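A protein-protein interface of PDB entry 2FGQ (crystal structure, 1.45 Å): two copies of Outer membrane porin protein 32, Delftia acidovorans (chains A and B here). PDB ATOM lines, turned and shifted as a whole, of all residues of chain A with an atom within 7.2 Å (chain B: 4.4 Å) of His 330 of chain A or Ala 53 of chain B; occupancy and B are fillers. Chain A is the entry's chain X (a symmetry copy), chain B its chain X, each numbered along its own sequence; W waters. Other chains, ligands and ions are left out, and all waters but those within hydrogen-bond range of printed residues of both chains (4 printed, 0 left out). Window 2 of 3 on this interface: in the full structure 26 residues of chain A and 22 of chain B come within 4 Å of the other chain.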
ATOM      1  N   GLY A   8     -11.721  17.332  -0.968  1.00  0.00           N
ATOM      2  CA  GLY A   8     -12.503  18.200  -0.135  1.00  0.00           C
ATOM      3  C   GLY A   8     -13.862  18.478  -0.695  1.00  0.00           C
ATOM      4  O   GLY A   8     -14.251  17.993  -1.765  1.00  0.00           O
ATOM      5  N   ILE A   9     -14.592  19.250   0.096  1.00  0.00           N
ATOM      6  CA  ILE A   9     -15.923  19.735  -0.243  1.00  0.00           C
ATOM      7  C   ILE A   9     -16.074  21.128   0.322  1.00  0.00           C
ATOM      8  O   ILE A   9     -15.822  21.356   1.488  1.00  0.00           O
ATOM      9  CB  ILE A   9     -17.088  18.841   0.321  1.00  0.00           C
ATOM     10  CG1 ILE A   9     -16.931  17.383  -0.089  1.00  0.00           C
ATOM     11  CG2 ILE A   9     -18.425  19.408  -0.105  1.00  0.00           C
ATOM     12  CD1 ILE A   9     -17.996  16.456   0.456  1.00  0.00           C
ATOM     13  N   VAL A  10     -16.538  22.060  -0.508  1.00  0.00           N
ATOM     14  CA  VAL A  10     -17.008  23.344   0.001  1.00  0.00           C
ATOM     15  C   VAL A  10     -18.525  23.401  -0.272  1.00  0.00           C
ATOM     16  O   VAL A  10     -18.963  23.395  -1.425  1.00  0.00           O
ATOM     17  CB  VAL A  10     -16.298  24.565  -0.604  1.00  0.00           C
ATOM     18  CG1 VAL A  10     -16.800  25.807   0.074  1.00  0.00           C
ATOM     19  CG2 VAL A  10     -14.809  24.448  -0.446  1.00  0.00           C
ATOM     20  N   ASP A  11     -19.280  23.436   0.802  1.00  0.00           N
ATOM     21  CA  ASP A  11     -20.743  23.475   0.771  1.00  0.00           C
ATOM     22  C   ASP A  11     -21.129  24.707   1.589  1.00  0.00           C
ATOM     23  O   ASP A  11     -20.886  24.770   2.804  1.00  0.00           O
ATOM     24  CB  ASP A  11     -21.314  22.186   1.358  1.00  0.00           C
ATOM     25  CG  ASP A  11     -22.808  22.185   1.455  1.00  0.00           C
ATOM     26  OD1 ASP A  11     -23.408  23.256   1.756  1.00  0.00           O
ATOM     27  OD2 ASP A  11     -23.443  21.116   1.294  1.00  0.00           O
ATOM     28  N   THR A  12     -21.664  25.711   0.890  1.00  0.00           N
ATOM     29  CA  THR A  12     -22.033  26.988   1.491  1.00  0.00           C
ATOM     30  C   THR A  12     -23.427  27.352   1.026  1.00  0.00           C
ATOM     31  O   THR A  12     -23.806  27.078  -0.115  1.00  0.00           O
ATOM     32  CB  THR A  12     -20.973  28.045   1.136  1.00  0.00           C
ATOM     33  OG1 THR A  12     -19.727  27.618   1.669  1.00  0.00           O
ATOM     34  CG2 THR A  12     -21.219  29.381   1.798  1.00  0.00           C
ATOM     35  N   ARG A  38     -15.284  20.042   3.964  1.00  0.00           N
ATOM     36  CA  ARG A  38     -14.077  19.411   4.486  1.00  0.00           C
ATOM     37  C   ARG A  38     -12.892  19.606   3.582  1.00  0.00           C
ATOM     38  O   ARG A  38     -13.031  19.921   2.397  1.00  0.00           O
ATOM     39  CB  ARG A  38     -14.344  17.893   4.661  1.00  0.00           C
ATOM     40  CG  ARG A  38     -14.411  17.119   3.357  1.00  0.00           C
ATOM     41  CD  ARG A  38     -15.130  15.765   3.462  1.00  0.00           C
ATOM     42  NE  ARG A  38     -16.532  15.966   3.731  1.00  0.00           N
ATOM     43  CZ  ARG A  38     -17.428  14.999   3.840  1.00  0.00           C
ATOM     44  NH1 ARG A  38     -17.053  13.720   3.785  1.00  0.00           N
ATOM     45  NH2 ARG A  38     -18.708  15.302   4.009  1.00  0.00           N
ATOM     46  N   LEU A 282     -25.314  19.608 -11.114  1.00  0.00           N
ATOM     47  CA  LEU A 282     -24.799  20.294 -12.307  1.00  0.00           C
ATOM     48  C   LEU A 282     -23.698  19.479 -12.943  1.00  0.00           C
ATOM     49  O   LEU A 282     -23.441  19.603 -14.150  1.00  0.00           O
ATOM     50  CB  LEU A 282     -24.273  21.669 -11.948  1.00  0.00           C
ATOM     51  CG  LEU A 282     -25.253  22.651 -11.313  1.00  0.00           C
ATOM     52  CD1 LEU A 282     -24.501  23.915 -10.940  1.00  0.00           C
ATOM     53  CD2 LEU A 282     -26.391  22.961 -12.274  1.00  0.00           C
ATOM     54  N   SER A 283     -23.083  18.625 -12.133  1.00  0.00           N
ATOM     55  CA  SER A 283     -22.088  17.669 -12.565  1.00  0.00           C
ATOM     56  C   SER A 283     -22.006  16.630 -11.463  1.00  0.00           C
ATOM     57  O   SER A 283     -22.651  16.774 -10.425  1.00  0.00           O
ATOM     58  CB  SER A 283     -20.714  18.338 -12.722  1.00  0.00           C
ATOM     59  OG  SER A 283     -20.152  18.733 -11.454  1.00  0.00           O
ATOM     60  N   ARG A 285     -19.593  16.388  -9.428  1.00  0.00           N
ATOM     61  CA  ARG A 285     -18.961  17.024  -8.279  1.00  0.00           C
ATOM     62  C   ARG A 285     -19.655  18.269  -7.764  1.00  0.00           C
ATOM     63  O   ARG A 285     -19.380  18.696  -6.665  1.00  0.00           O
ATOM     64  CB  ARG A 285     -17.493  17.375  -8.604  1.00  0.00           C
ATOM     65  CG  ARG A 285     -16.539  16.158  -8.829  1.00  0.00           C
ATOM     66  CD  ARG A 285     -15.242  16.513  -9.669  1.00  0.00           C
ATOM     67  NE  ARG A 285     -14.679  17.722  -9.115  1.00  0.00           N
ATOM     68  CZ  ARG A 285     -13.941  18.605  -9.726  1.00  0.00           C
ATOM     69  NH1 ARG A 285     -13.574  18.465 -11.008  1.00  0.00           N
ATOM     70  NH2 ARG A 285     -13.536  19.648  -9.020  1.00  0.00           N
ATOM     71  N   THR A 286     -20.549  18.860  -8.544  1.00  0.00           N
ATOM     72  CA  THR A 286     -21.173  20.131  -8.154  1.00  0.00           C
ATOM     73  C   THR A 286     -22.713  20.016  -8.167  1.00  0.00           C
ATOM     74  O   THR A 286     -23.292  19.611  -9.171  1.00  0.00           O
ATOM     75  CB  THR A 286     -20.781  21.223  -9.136  1.00  0.00           C
ATOM     76  OG1 THR A 286     -19.352  21.385  -9.085  1.00  0.00           O
ATOM     77  CG2 THR A 286     -21.363  22.535  -8.712  1.00  0.00           C
ATOM     78  N   ALA A 287     -23.351  20.372  -7.062  1.00  0.00           N
ATOM     79  CA  ALA A 287     -24.811  20.335  -6.955  1.00  0.00           C
ATOM     80  C   ALA A 287     -25.334  21.591  -6.310  1.00  0.00           C
ATOM     81  O   ALA A 287     -24.674  22.207  -5.479  1.00  0.00           O
ATOM     82  CB  ALA A 287     -25.239  19.138  -6.116  1.00  0.00           C
ATOM     83  N   TYR A 289     -28.727  22.746  -4.028  1.00  0.00           N
ATOM     84  CA  TYR A 289     -29.656  22.049  -3.166  1.00  0.00           C
ATOM     85  C   TYR A 289     -30.516  22.983  -2.371  1.00  0.00           C
ATOM     86  O   TYR A 289     -30.207  24.151  -2.193  1.00  0.00           O
ATOM     87  CB  TYR A 289     -28.911  21.095  -2.207  1.00  0.00           C
ATOM     88  CG  TYR A 289     -28.057  21.822  -1.179  1.00  0.00           C
ATOM     89  CD1 TYR A 289     -26.715  22.083  -1.402  1.00  0.00           C
ATOM     90  CD2 TYR A 289     -28.605  22.263   0.007  1.00  0.00           C
ATOM     91  CE1 TYR A 289     -25.947  22.781  -0.468  1.00  0.00           C
ATOM     92  CE2 TYR A 289     -27.853  22.970   0.938  1.00  0.00           C
ATOM     93  CZ  TYR A 289     -26.508  23.187   0.727  1.00  0.00           C
ATOM     94  OH  TYR A 289     -25.773  23.840   1.687  1.00  0.00           O
ATOM     95  N   ILE A 328     -24.898  25.518  -2.514  1.00  0.00           N
ATOM     96  CA  ILE A 328     -24.112  24.838  -3.519  1.00  0.00           C
ATOM     97  C   ILE A 328     -23.127  23.960  -2.772  1.00  0.00           C
ATOM     98  O   ILE A 328     -22.545  24.362  -1.753  1.00  0.00           O
ATOM     99  CB  ILE A 328     -23.389  25.856  -4.456  1.00  0.00           C
ATOM    100  CG1 ILE A 328     -22.534  25.138  -5.517  1.00  0.00           C
ATOM    101  CG2 ILE A 328     -22.525  26.846  -3.724  1.00  0.00           C
ATOM    102  CD1 ILE A 328     -22.074  26.024  -6.659  1.00  0.00           C
ATOM    103  N   ARG A 329     -22.934  22.764  -3.312  1.00  0.00           N
ATOM    104  CA  ARG A 329     -21.913  21.861  -2.803  1.00  0.00           C
ATOM    105  C   ARG A 329     -20.952  21.565  -3.942  1.00  0.00           C
ATOM    106  O   ARG A 329     -21.362  21.110  -5.010  1.00  0.00           O
ATOM    107  CB  ARG A 329     -22.605  20.582  -2.337  1.00  0.00           C
ATOM    108  CG  ARG A 329     -21.655  19.466  -2.039  1.00  0.00           C
ATOM    109  CD  ARG A 329     -22.006  18.304  -2.981  1.00  0.00           C
ATOM    110  NE  ARG A 329     -22.844  17.625  -2.140  1.00  0.00           N
ATOM    111  CZ  ARG A 329     -23.857  16.743  -2.334  1.00  0.00           C
ATOM    112  NH1 ARG A 329     -24.389  16.278  -3.496  1.00  0.00           N
ATOM    113  NH2 ARG A 329     -24.361  16.280  -1.213  1.00  0.00           N
ATOM    114  N   HIS A 330     -19.667  21.792  -3.716  1.00  0.00           N
ATOM    115  CA  HIS A 330     -18.646  21.555  -4.720  1.00  0.00           C
ATOM    116  C   HIS A 330     -17.576  20.650  -4.112  1.00  0.00           C
ATOM    117  O   HIS A 330     -16.865  21.042  -3.176  1.00  0.00           O
ATOM    118  CB  HIS A 330     -18.004  22.829  -5.208  1.00  0.00           C
ATOM    119  CG  HIS A 330     -17.010  22.580  -6.277  1.00  0.00           C
ATOM    120  ND1 HIS A 330     -15.649  22.760  -6.121  1.00  0.00           N
ATOM    121  CD2 HIS A 330     -17.185  22.089  -7.521  1.00  0.00           C
ATOM    122  CE1 HIS A 330     -15.043  22.402  -7.251  1.00  0.00           C
ATOM    123  NE2 HIS A 330     -15.955  22.022  -8.120  1.00  0.00           N
ATOM    124  N   ALA A 331     -17.456  19.469  -4.681  1.00  0.00           N
ATOM    125  CA  ALA A 331     -16.442  18.485  -4.264  1.00  0.00           C
ATOM    126  C   ALA A 331     -15.235  18.594  -5.165  1.00  0.00           C
ATOM    127  O   ALA A 331     -15.364  18.914  -6.346  1.00  0.00           O
ATOM    128  CB  ALA A 331     -17.007  17.074  -4.347  1.00  0.00           C
ATOM    129  N   PHE A 332     -14.059  18.293  -4.607  1.00  0.00           N
ATOM    130  CA  PHE A 332     -12.837  18.271  -5.390  1.00  0.00           C
ATOM    131  C   PHE A 332     -11.917  17.156  -4.918  1.00  0.00           C
ATOM    132  O   PHE A 332     -12.116  16.566  -3.844  1.00  0.00           O
ATOM    133  CB  PHE A 332     -12.144  19.628  -5.364  1.00  0.00           C
ATOM    134  CG  PHE A 332     -11.786  20.125  -3.989  1.00  0.00           C
ATOM    135  CD1 PHE A 332     -10.536  19.848  -3.428  1.00  0.00           C
ATOM    136  CD2 PHE A 332     -12.660  20.894  -3.256  1.00  0.00           C
ATOM    137  CE1 PHE A 332     -10.197  20.312  -2.171  1.00  0.00           C
ATOM    138  CE2 PHE A 332     -12.315  21.344  -1.986  1.00  0.00           C
ATOM    139  CZ  PHE A 332     -11.056  21.033  -1.454  1.00  0.00           C
ATOM    140  OXT PHE A 332     -10.986  16.838  -5.683  1.00  0.00           O
ATOM    141  N   GLY B  43      -9.547  25.788  -7.231  1.00  0.00           N
ATOM    142  CA  GLY B  43      -9.849  24.941  -8.350  1.00  0.00           C
ATOM    143  C   GLY B  43     -10.993  25.476  -9.154  1.00  0.00           C
ATOM    144  O   GLY B  43     -11.771  26.279  -8.677  1.00  0.00           O
ATOM    145  N   THR B  44     -11.070  24.991 -10.382  1.00  0.00           N
ATOM    146  CA  THR B  44     -12.123  25.367 -11.285  1.00  0.00           C
ATOM    147  C   THR B  44     -12.587  24.090 -11.980  1.00  0.00           C
ATOM    148  O   THR B  44     -11.775  23.232 -12.324  1.00  0.00           O
ATOM    149  CB  THR B  44     -11.615  26.408 -12.351  1.00  0.00           C
ATOM    150  OG1 THR B  44     -11.282  27.644 -11.705  1.00  0.00           O
ATOM    151  CG2 THR B  44     -12.676  26.820 -13.230  1.00  0.00           C
ATOM    152  N   GLU B  45     -13.884  23.959 -12.181  1.00  0.00           N
ATOM    153  CA  GLU B  45     -14.459  22.832 -12.884  1.00  0.00           C
ATOM    154  C   GLU B  45     -15.358  23.363 -14.005  1.00  0.00           C
ATOM    155  O   GLU B  45     -16.241  24.149 -13.759  1.00  0.00           O
ATOM    156  CB  GLU B  45     -15.341  22.023 -11.936  1.00  0.00           C
ATOM    157  CG  GLU B  45     -15.992  20.814 -12.594  1.00  0.00           C
ATOM    158  CD  GLU B  45     -17.058  20.130 -11.736  1.00  0.00           C
ATOM    159  OE1 GLU B  45     -17.326  20.602 -10.613  1.00  0.00           O
ATOM    160  OE2 GLU B  45     -17.655  19.124 -12.207  1.00  0.00           O
ATOM    161  N   LEU B  47     -18.436  23.003 -16.197  1.00  0.00           N
ATOM    162  CA  LEU B  47     -19.718  22.335 -16.058  1.00  0.00           C
ATOM    163  C   LEU B  47     -20.428  22.193 -17.384  1.00  0.00           C
ATOM    164  O   LEU B  47     -21.503  21.606 -17.436  1.00  0.00           O
ATOM    165  CB  LEU B  47     -20.637  23.080 -15.094  1.00  0.00           C
ATOM    166  CG  LEU B  47     -20.066  23.291 -13.679  1.00  0.00           C
ATOM    167  CD1 LEU B  47     -21.019  24.127 -12.842  1.00  0.00           C
ATOM    168  CD2 LEU B  47     -19.821  21.985 -13.004  1.00  0.00           C
ATOM    169  N   LYS B  52     -18.833  27.512 -15.059  1.00  0.00           N
ATOM    170  CA  LYS B  52     -17.727  26.944 -14.302  1.00  0.00           C
ATOM    171  C   LYS B  52     -18.032  27.059 -12.801  1.00  0.00           C
ATOM    172  O   LYS B  52     -18.633  28.024 -12.354  1.00  0.00           O
ATOM    173  CB  LYS B  52     -16.431  27.692 -14.588  1.00  0.00           C
ATOM    174  CG  LYS B  52     -15.926  27.558 -16.008  1.00  0.00           C
ATOM    175  CD  LYS B  52     -14.551  28.215 -16.136  1.00  0.00           C
ATOM    176  CE  LYS B  52     -14.103  28.320 -17.613  1.00  0.00           C
ATOM    177  NZ  LYS B  52     -14.262  27.023 -18.347  1.00  0.00           N
ATOM    178  N   ALA B  53     -17.651  26.044 -12.044  1.00  0.00           N
ATOM    179  CA  ALA B  53     -17.684  26.106 -10.601  1.00  0.00           C
ATOM    180  C   ALA B  53     -16.271  26.281 -10.103  1.00  0.00           C
ATOM    181  O   ALA B  53     -15.332  25.758 -10.681  1.00  0.00           O
ATOM    182  CB  ALA B  53     -18.271  24.843 -10.026  1.00  0.00           C
ATOM    183  N   GLY B  54     -16.126  26.976  -8.994  1.00  0.00           N
ATOM    184  CA  GLY B  54     -14.795  27.185  -8.424  1.00  0.00           C
ATOM    185  C   GLY B  54     -14.834  27.124  -6.926  1.00  0.00           C
ATOM    186  O   GLY B  54     -15.862  27.272  -6.304  1.00  0.00           O
ATOM    187  N   PHE B  55     -13.651  26.940  -6.338  1.00  0.00           N
ATOM    188  CA  PHE B  55     -13.485  27.160  -4.924  1.00  0.00           C
ATOM    189  C   PHE B  55     -12.097  27.750  -4.691  1.00  0.00           C
ATOM    190  O   PHE B  55     -11.228  27.629  -5.540  1.00  0.00           O
ATOM    191  CB  PHE B  55     -13.676  25.856  -4.134  1.00  0.00           C
ATOM    192  CG  PHE B  55     -12.495  24.966  -4.166  1.00  0.00           C
ATOM    193  CD1 PHE B  55     -11.528  25.030  -3.170  1.00  0.00           C
ATOM    194  CD2 PHE B  55     -12.258  24.144  -5.261  1.00  0.00           C
ATOM    195  CE1 PHE B  55     -10.386  24.269  -3.240  1.00  0.00           C
ATOM    196  CE2 PHE B  55     -11.087  23.343  -5.309  1.00  0.00           C
ATOM    197  CZ  PHE B  55     -10.167  23.431  -4.290  1.00  0.00           C
ATOM    198  N   VAL B  79     -16.765  29.567  -2.580  1.00  0.00           N
ATOM    199  CA  VAL B  79     -17.227  28.706  -3.662  1.00  0.00           C
ATOM    200  C   VAL B  79     -17.976  29.619  -4.622  1.00  0.00           C
ATOM    201  O   VAL B  79     -18.594  30.605  -4.214  1.00  0.00           O
ATOM    202  CB  VAL B  79     -18.081  27.521  -3.117  1.00  0.00           C
ATOM    203  CG1 VAL B  79     -19.311  27.975  -2.285  1.00  0.00           C
ATOM    204  CG2 VAL B  79     -18.512  26.571  -4.235  1.00  0.00           C
ATOM    205  N   SER B  80     -17.876  29.299  -5.903  1.00  0.00           N
ATOM    206  CA  SER B  80     -18.387  30.223  -6.907  1.00  0.00           C
ATOM    207  C   SER B  80     -18.968  29.542  -8.118  1.00  0.00           C
ATOM    208  O   SER B  80     -18.660  28.408  -8.418  1.00  0.00           O
ATOM    209  CB  SER B  80     -17.282  31.164  -7.399  1.00  0.00           C
ATOM    210  OG  SER B  80     -16.196  30.421  -7.943  1.00  0.00           O
ATOM    211  N   LEU B  81     -19.750  30.310  -8.854  1.00  0.00           N
ATOM    212  CA  LEU B  81     -20.137  29.973 -10.215  1.00  0.00           C
ATOM    213  C   LEU B  81     -19.793  31.151 -11.099  1.00  0.00           C
ATOM    214  O   LEU B  81     -19.961  32.279 -10.699  1.00  0.00           O
ATOM    215  CB  LEU B  81     -21.645  29.688 -10.318  1.00  0.00           C
ATOM    216  CG  LEU B  81     -22.177  28.398  -9.731  1.00  0.00           C
ATOM    217  CD1 LEU B  81     -23.710  28.399  -9.886  1.00  0.00           C
ATOM    218  CD2 LEU B  81     -21.563  27.165 -10.379  1.00  0.00           C
HETATM  219  O   HOH W   1     -11.967  20.403 -13.244  1.00  0.00           O
HETATM  220  O   HOH W   2     -17.894  16.428 -11.890  1.00  0.00           O
HETATM  221  O   HOH W   3     -21.805  19.035 -16.142  1.00  0.00           O
HETATM  222  O   HOH W   4     -24.590  21.649 -16.018  1.00  0.00           O
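OE1 of Glu 45 of chain B sits at hydrogen-bond distance from OG1 of Thr 286 of chain A (2.7 Å).
A ring nitrogen (NE2) of His 330 of chain A is in hydrogen-bond range of the side-chain carboxylate (OE1) of Glu 45 of chain B (3.2 Å).
OG of Ser 283 of chain A lies within hydrogen-bond range of OE2 of Glu 45 of chain B, 2.6 Å away.
The backbone NH (N) of Gly 43 of chain B is in hydrogen-bond range of the backbone carbonyl oxygen (O) of Phe 55 of chain B, at 3.0 Å.
The backbone carbonyl oxygen (O) of Gly 8 of chain A is in hydrogen-bond range of the backbone NH (N) of Phe 332 of chain A.
O of His 330 of chain A is in hydrogen-bond range of N of Val 10 of chain A, at 2.9 Å.
The backbone NH (N) of Glu 45 of chain B is in hydrogen-bond range of the backbone carbonyl oxygen (O) of Ala 53 of chain B, at 2.8 Å.
The side-chain hydroxyl (OG) of Ser 283 of chain A sits at hydrogen-bond distance from the backbone NH (N) of Thr 286 of chain A (2.9 Å).
The backbone NH (N) of Arg 285 of chain A sits at hydrogen-bond distance from the side-chain hydroxyl (OG) of Ser 283 of chain A (3.1 Å).
Val 10 of chain A touches Val 79 of chain B (CG1 to CB, 3.8 Å).
CB of Thr 12 of chain A touches CG1 of Val 79 of chain B, at 3.8 Å.
Leu 47 of chain B touches Leu 282 of chain A.
Glu 45 of chain B touches Arg 285 of chain A.
OG1 of Thr 286 of chain A touches CD2 of Leu 47 of chain B, 3.99 Å away.
Thr 286 of chain A touches Ala 53 of chain B.
Ile 328 of chain A touches Val 79 of chain B.
Ile 328 of chain A touches Leu 81 of chain B.
Phe 55 of chain B touches His 330 of chain A (CD2 to ND1, 3.8 Å).
His 330 of chain A touches Val 79 of chain B.
Of the printed residues of chain B, Val 10 of chain A touches Val 79.
Of the printed residues of chain B, Leu 282 of chain A touches Leu 47.
Of chain B, only Glu 45, Ala 53, Phe 55 and Val 79 come within 4 Å of His 330 of chain A.
Printed residues of chain A within 4 Å of Glu 45 of chain B: Ser 283, Arg 285, Thr 286 and His 330.
Printed residues of chain A within 4 Å of Leu 47 of chain B: Leu 282, Ser 283 and Thr 286.
Printed residues of chain A within 4 Å of Ala 53 of chain B: Thr 286 and His 330.
The nearest printed residue of chain B that does not touch His 330 of chain A is Gly 54 of chain B (4.5 Å).
The nearest printed residue of chain B that does not touch Thr 286 of chain A is Leu 81 of chain B (4.9 Å).
Printed residues of chain A that touch a printed residue of chain B: Val 10, Thr 12, Leu 282, Ser 283, Arg 285, Thr 286, Ile 328, His 330 and Phe 332.
Hydrophobic or aromatic side chains of chain B that line the printed part of chain A: Leu 47, Ala 53, Phe 55, Val 79 and Leu 81.
Among the printed residues, 16 pairs touch across the chains.
Among the printed residues, no Asp or Glu carboxylate lies within 4 Å of a Lys or Arg side-chain nitrogen of the other chain.
No position is printed for both chains.
Water W3 bridges the backbone carbonyl oxygen of Leu 282 of chain A (2.6 Å) and the backbone carbonyl oxygen of Leu 47 of chain B (2.9 Å).
Water W2 lies within hydrogen-bond range of OE2 of Glu 45 of chain B (2.7 Å), N of Arg 285 of chain A (3.0 Å) and OG of Ser 283 of chain A (3.3 Å).
Water W1 lies within hydrogen-bond range of the backbone carbonyl oxygen (O) of Thr 44 of chain B (3.0 Å) and the guanidinium group (NH1) of Arg 285 of chain A (3.4 Å).
Water W4 lies within hydrogen-bond range of O of Leu 282 of chain A (3.0 Å) and O of Leu 47 of chain B (3.4 Å).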
